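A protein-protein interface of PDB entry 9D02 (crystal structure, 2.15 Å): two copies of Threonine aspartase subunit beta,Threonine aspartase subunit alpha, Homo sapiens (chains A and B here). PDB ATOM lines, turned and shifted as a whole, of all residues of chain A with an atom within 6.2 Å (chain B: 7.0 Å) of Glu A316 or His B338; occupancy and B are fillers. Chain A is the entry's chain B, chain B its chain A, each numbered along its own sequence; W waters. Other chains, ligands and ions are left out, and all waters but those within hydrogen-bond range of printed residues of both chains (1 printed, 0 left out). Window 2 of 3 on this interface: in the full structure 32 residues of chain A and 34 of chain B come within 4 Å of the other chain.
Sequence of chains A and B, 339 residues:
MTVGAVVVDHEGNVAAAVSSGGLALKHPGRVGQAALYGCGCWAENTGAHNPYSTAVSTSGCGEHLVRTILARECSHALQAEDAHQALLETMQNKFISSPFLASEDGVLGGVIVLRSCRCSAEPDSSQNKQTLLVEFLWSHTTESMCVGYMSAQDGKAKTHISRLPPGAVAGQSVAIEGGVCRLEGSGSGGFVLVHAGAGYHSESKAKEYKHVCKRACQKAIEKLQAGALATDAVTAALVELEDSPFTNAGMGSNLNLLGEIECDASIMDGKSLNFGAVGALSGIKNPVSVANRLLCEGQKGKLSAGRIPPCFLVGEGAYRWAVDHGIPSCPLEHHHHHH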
ATOM      1  N   ALA A 280       3.047  -1.849  -2.826  1.00  0.00           N
ATOM      2  CA  ALA A 280       3.581  -2.912  -1.978  1.00  0.00           C
ATOM      3  C   ALA A 280       3.616  -2.480  -0.513  1.00  0.00           C
ATOM      4  O   ALA A 280       4.620  -2.650   0.189  1.00  0.00           O
ATOM      5  CB  ALA A 280       4.972  -3.356  -2.462  1.00  0.00           C
ATOM      6  N   VAL A 314       7.000   3.184  -1.719  1.00  0.00           N
ATOM      7  CA  VAL A 314       6.737   1.750  -1.715  1.00  0.00           C
ATOM      8  C   VAL A 314       7.348   1.078  -0.490  1.00  0.00           C
ATOM      9  O   VAL A 314       8.285   1.587   0.134  1.00  0.00           O
ATOM     10  CB  VAL A 314       7.249   1.056  -2.994  1.00  0.00           C
ATOM     11  CG1 VAL A 314       6.597   1.661  -4.232  1.00  0.00           C
ATOM     12  CG2 VAL A 314       8.791   1.120  -3.074  1.00  0.00           C
ATOM     13  N   GLY A 315       6.781  -0.089  -0.155  1.00  0.00           N
ATOM     14  CA  GLY A 315       7.413  -1.053   0.737  1.00  0.00           C
ATOM     15  C   GLY A 315       7.611  -0.540   2.149  1.00  0.00           C
ATOM     16  O   GLY A 315       6.793   0.212   2.684  1.00  0.00           O
ATOM     17  N   GLU A 316       8.710  -0.978   2.774  1.00  0.00           N
ATOM     18  CA  GLU A 316       9.010  -0.571   4.146  1.00  0.00           C
ATOM     19  C   GLU A 316       9.081   0.957   4.268  1.00  0.00           C
ATOM     20  O   GLU A 316       8.612   1.532   5.256  1.00  0.00           O
ATOM     21  CB  GLU A 316      10.310  -1.223   4.598  1.00  0.00           C
ATOM     22  CG  GLU A 316      10.684  -0.954   6.053  1.00  0.00           C
ATOM     23  CD  GLU A 316       9.644  -1.499   7.038  1.00  0.00           C
ATOM     24  OE1 GLU A 316       8.872  -2.413   6.659  1.00  0.00           O
ATOM     25  OE2 GLU A 316       9.607  -1.012   8.191  1.00  0.00           O
ATOM     26  N   GLY A 317       9.664   1.633   3.275  1.00  0.00           N
ATOM     27  CA  GLY A 317       9.739   3.084   3.344  1.00  0.00           C
ATOM     28  C   GLY A 317       8.374   3.746   3.397  1.00  0.00           C
ATOM     29  O   GLY A 317       8.167   4.698   4.152  1.00  0.00           O
ATOM     30  N   ALA A 318       7.419   3.243   2.612  1.00  0.00           N
ATOM     31  CA  ALA A 318       6.061   3.772   2.683  1.00  0.00           C
ATOM     32  C   ALA A 318       5.429   3.513   4.050  1.00  0.00           C
ATOM     33  O   ALA A 318       4.720   4.373   4.583  1.00  0.00           O
ATOM     34  CB  ALA A 318       5.194   3.163   1.579  1.00  0.00           C
ATOM     35  N   TYR A 319       5.656   2.333   4.633  1.00  0.00           N
ATOM     36  CA  TYR A 319       5.111   2.069   5.962  1.00  0.00           C
ATOM     37  C   TYR A 319       5.677   3.059   6.983  1.00  0.00           C
ATOM     38  O   TYR A 319       4.927   3.685   7.746  1.00  0.00           O
ATOM     39  CB  TYR A 319       5.396   0.614   6.373  1.00  0.00           C
ATOM     40  CG  TYR A 319       5.028   0.273   7.804  1.00  0.00           C
ATOM     41  CD1 TYR A 319       5.996   0.281   8.806  1.00  0.00           C
ATOM     42  CD2 TYR A 319       3.711  -0.049   8.164  1.00  0.00           C
ATOM     43  CE1 TYR A 319       5.676  -0.035  10.139  1.00  0.00           C
ATOM     44  CE2 TYR A 319       3.380  -0.378   9.508  1.00  0.00           C
ATOM     45  CZ  TYR A 319       4.369  -0.358  10.481  1.00  0.00           C
ATOM     46  OH  TYR A 319       4.067  -0.662  11.794  1.00  0.00           O
ATOM     47  N   ARG A 320       7.001   3.236   6.994  1.00  0.00           N
ATOM     48  CA  ARG A 320       7.615   4.134   7.972  1.00  0.00           C
ATOM     49  C   ARG A 320       7.109   5.563   7.811  1.00  0.00           C
ATOM     50  O   ARG A 320       6.860   6.254   8.804  1.00  0.00           O
ATOM     51  CB  ARG A 320       9.134   4.088   7.843  1.00  0.00           C
ATOM     52  CG  ARG A 320       9.727   2.733   8.206  1.00  0.00           C
ATOM     53  CD  ARG A 320      10.461   2.791   9.533  1.00  0.00           C
ATOM     54  NE  ARG A 320       9.659   3.412  10.583  1.00  0.00           N
ATOM     55  CZ  ARG A 320       8.960   2.740  11.492  1.00  0.00           C
ATOM     56  NH1 ARG A 320       8.957   1.414  11.487  1.00  0.00           N
ATOM     57  NH2 ARG A 320       8.265   3.395  12.411  1.00  0.00           N
ATOM     58  N   TRP A 321       6.950   6.020   6.565  1.00  0.00           N
ATOM     59  CA  TRP A 321       6.392   7.345   6.324  1.00  0.00           C
ATOM     60  C   TRP A 321       4.961   7.441   6.842  1.00  0.00           C
ATOM     61  O   TRP A 321       4.576   8.446   7.449  1.00  0.00           O
ATOM     62  CB  TRP A 321       6.447   7.655   4.829  1.00  0.00           C
ATOM     63  CG  TRP A 321       6.176   9.087   4.431  1.00  0.00           C
ATOM     64  CD1 TRP A 321       7.106  10.059   4.182  1.00  0.00           C
ATOM     65  CD2 TRP A 321       4.894   9.692   4.198  1.00  0.00           C
ATOM     66  NE1 TRP A 321       6.480  11.230   3.814  1.00  0.00           N
ATOM     67  CE2 TRP A 321       5.127  11.035   3.822  1.00  0.00           C
ATOM     68  CE3 TRP A 321       3.576   9.236   4.289  1.00  0.00           C
ATOM     69  CZ2 TRP A 321       4.088  11.926   3.541  1.00  0.00           C
ATOM     70  CZ3 TRP A 321       2.539  10.123   3.999  1.00  0.00           C
ATOM     71  CH2 TRP A 321       2.805  11.453   3.630  1.00  0.00           C
ATOM     72  N   HIS B  27      13.395  10.226   0.772  1.00  0.00           N
ATOM     73  CA  HIS B  27      12.858   9.326   1.778  1.00  0.00           C
ATOM     74  C   HIS B  27      12.976   7.885   1.288  1.00  0.00           C
ATOM     75  O   HIS B  27      12.773   7.615   0.099  1.00  0.00           O
ATOM     76  CB  HIS B  27      11.394   9.673   2.087  1.00  0.00           C
ATOM     77  CG  HIS B  27      10.834   8.942   3.272  1.00  0.00           C
ATOM     78  ND1 HIS B  27      10.358   7.650   3.192  1.00  0.00           N
ATOM     79  CD2 HIS B  27      10.708   9.308   4.572  1.00  0.00           C
ATOM     80  CE1 HIS B  27       9.939   7.262   4.385  1.00  0.00           C
ATOM     81  NE2 HIS B  27      10.138   8.250   5.239  1.00  0.00           N
ATOM     82  N   PRO B  28      13.310   6.940   2.164  1.00  0.00           N
ATOM     83  CA  PRO B  28      13.346   5.533   1.744  1.00  0.00           C
ATOM     84  C   PRO B  28      12.047   5.144   1.062  1.00  0.00           C
ATOM     85  O   PRO B  28      10.962   5.583   1.457  1.00  0.00           O
ATOM     86  CB  PRO B  28      13.542   4.772   3.062  1.00  0.00           C
ATOM     87  CG  PRO B  28      14.245   5.758   3.946  1.00  0.00           C
ATOM     88  CD  PRO B  28      13.703   7.116   3.573  1.00  0.00           C
ATOM     89  N   GLY B  29      12.167   4.334   0.011  1.00  0.00           N
ATOM     90  CA  GLY B  29      11.001   3.867  -0.720  1.00  0.00           C
ATOM     91  C   GLY B  29      10.464   4.826  -1.767  1.00  0.00           C
ATOM     92  O   GLY B  29       9.473   4.495  -2.437  1.00  0.00           O
ATOM     93  N   GLY B 315      11.594  -3.072  -3.891  1.00  0.00           N
ATOM     94  CA  GLY B 315      12.005  -3.276  -2.509  1.00  0.00           C
ATOM     95  C   GLY B 315      12.533  -4.667  -2.247  1.00  0.00           C
ATOM     96  O   GLY B 315      13.231  -5.262  -3.079  1.00  0.00           O
ATOM     97  N   GLU B 316      12.197  -5.192  -1.061  1.00  0.00           N
ATOM     98  CA  GLU B 316      12.691  -6.505  -0.647  1.00  0.00           C
ATOM     99  C   GLU B 316      12.339  -7.578  -1.660  1.00  0.00           C
ATOM    100  O   GLU B 316      13.196  -8.387  -2.044  1.00  0.00           O
ATOM    101  CB  GLU B 316      12.104  -6.869   0.712  1.00  0.00           C
ATOM    102  CG  GLU B 316      12.539  -8.235   1.265  1.00  0.00           C
ATOM    103  CD  GLU B 316      14.029  -8.331   1.506  1.00  0.00           C
ATOM    104  OE1 GLU B 316      14.553  -9.466   1.558  1.00  0.00           O
ATOM    105  OE2 GLU B 316      14.680  -7.273   1.656  1.00  0.00           O
ATOM    106  N   HIS B 335      19.535  -3.652   2.291  1.00  0.00           N
ATOM    107  CA  HIS B 335      18.875  -3.312   3.546  1.00  0.00           C
ATOM    108  C   HIS B 335      17.464  -3.883   3.556  1.00  0.00           C
ATOM    109  O   HIS B 335      16.749  -3.825   2.549  1.00  0.00           O
ATOM    110  CB  HIS B 335      18.849  -1.777   3.797  1.00  0.00           C
ATOM    111  CG  HIS B 335      18.242  -0.973   2.684  1.00  0.00           C
ATOM    112  ND1 HIS B 335      16.881  -0.908   2.461  1.00  0.00           N
ATOM    113  CD2 HIS B 335      18.811  -0.171   1.751  1.00  0.00           C
ATOM    114  CE1 HIS B 335      16.640  -0.116   1.432  1.00  0.00           C
ATOM    115  NE2 HIS B 335      17.794   0.343   0.981  1.00  0.00           N
ATOM    116  N   HIS B 336      17.081  -4.463   4.695  1.00  0.00           N
ATOM    117  CA  HIS B 336      15.745  -5.014   4.910  1.00  0.00           C
ATOM    118  C   HIS B 336      15.294  -4.562   6.292  1.00  0.00           C
ATOM    119  O   HIS B 336      15.493  -5.268   7.284  1.00  0.00           O
ATOM    120  CB  HIS B 336      15.722  -6.533   4.792  1.00  0.00           C
ATOM    121  CG  HIS B 336      14.361  -7.127   4.998  1.00  0.00           C
ATOM    122  ND1 HIS B 336      13.202  -6.473   4.633  1.00  0.00           N
ATOM    123  CD2 HIS B 336      13.974  -8.309   5.532  1.00  0.00           C
ATOM    124  CE1 HIS B 336      12.160  -7.227   4.933  1.00  0.00           C
ATOM    125  NE2 HIS B 336      12.601  -8.348   5.477  1.00  0.00           N
ATOM    126  N   HIS B 337      14.686  -3.384   6.351  1.00  0.00           N
ATOM    127  CA  HIS B 337      14.168  -2.876   7.608  1.00  0.00           C
ATOM    128  C   HIS B 337      12.812  -3.506   7.905  1.00  0.00           C
ATOM    129  O   HIS B 337      12.064  -3.881   6.997  1.00  0.00           O
ATOM    130  CB  HIS B 337      14.068  -1.351   7.561  1.00  0.00           C
ATOM    131  CG  HIS B 337      15.351  -0.678   7.172  1.00  0.00           C
ATOM    132  ND1 HIS B 337      16.486  -0.732   7.952  1.00  0.00           N
ATOM    133  CD2 HIS B 337      15.679   0.056   6.082  1.00  0.00           C
ATOM    134  CE1 HIS B 337      17.457  -0.057   7.362  1.00  0.00           C
ATOM    135  NE2 HIS B 337      16.993   0.432   6.226  1.00  0.00           N
ATOM    136  N   HIS B 338      12.511  -3.638   9.192  1.00  0.00           N
ATOM    137  CA  HIS B 338      11.319  -4.360   9.630  1.00  0.00           C
ATOM    138  C   HIS B 338      10.651  -3.695  10.836  1.00  0.00           C
ATOM    139  O   HIS B 338      10.977  -2.563  11.203  1.00  0.00           O
ATOM    140  CB  HIS B 338      11.679  -5.813   9.966  1.00  0.00           C
HETATM  141  O   HOH W   1      10.492  -3.099   0.835  1.00  0.00           O
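Ala A280 touches none of the printed residues of chain B. Of the printed residues of chain B, Val A314 touches Gly B29 (2.9 Å). Of chain B, only His B337 and His B338 come within 4 Å of Glu A316. Of the printed residues of chain B, Gly A317 touches His B27 and Pro B28. Of the printed residues of chain B, Trp A321 touches His B27. Printed residues of chain A within 4 Å of Gly B29: Val A314 (2.9 Å). His B335 touches none of the printed residues of chain A. Printed residues of chain A within 4 Å of His B337: Glu A316. His B338 touches one residue of chain A. The nearest printed residue of chain B that does not touch Gly A317 is Gly B29 (4.3 Å).
Of the 9 printed residues of chain B, 5 touch a printed residue of chain A. Hydrophobic or aromatic side chains of chain B within 4 Å of the printed part of chain A: His B27 and His B337. Printed residues of chain A that touch a printed residue of chain B: Val A314, Glu A316, Gly A317 and Trp A321. Hydrophobic or aromatic side chains of chain A that line the printed part of chain B: Val A314 and Trp A321. Among the printed residues, 6 pairs touch across the chains. Among the printed residues, no Asp or Glu carboxylate lies within 4 Å of a Lys or Arg side-chain nitrogen of the other chain.
Water W1 lies within hydrogen-bond range of N of Glu B316 and N of Glu A316.
The backbone carbonyl oxygen (O) of Gly B29 lies within hydrogen-bond range of the backbone NH (N) of Val A314 (2.9 Å).
Among the printed residues, merely in contact across the chains: Glu A316 with His B337, Glu A316 with His B338, Gly A317 with His B27, Gly A317 with Pro B28 and Trp A321 with His B27.
Positions printed for both chains: 315 and 316. Of the 6 pairs that touch across the chains among the printed residues, none has its exchanged pair printed and touching as well.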
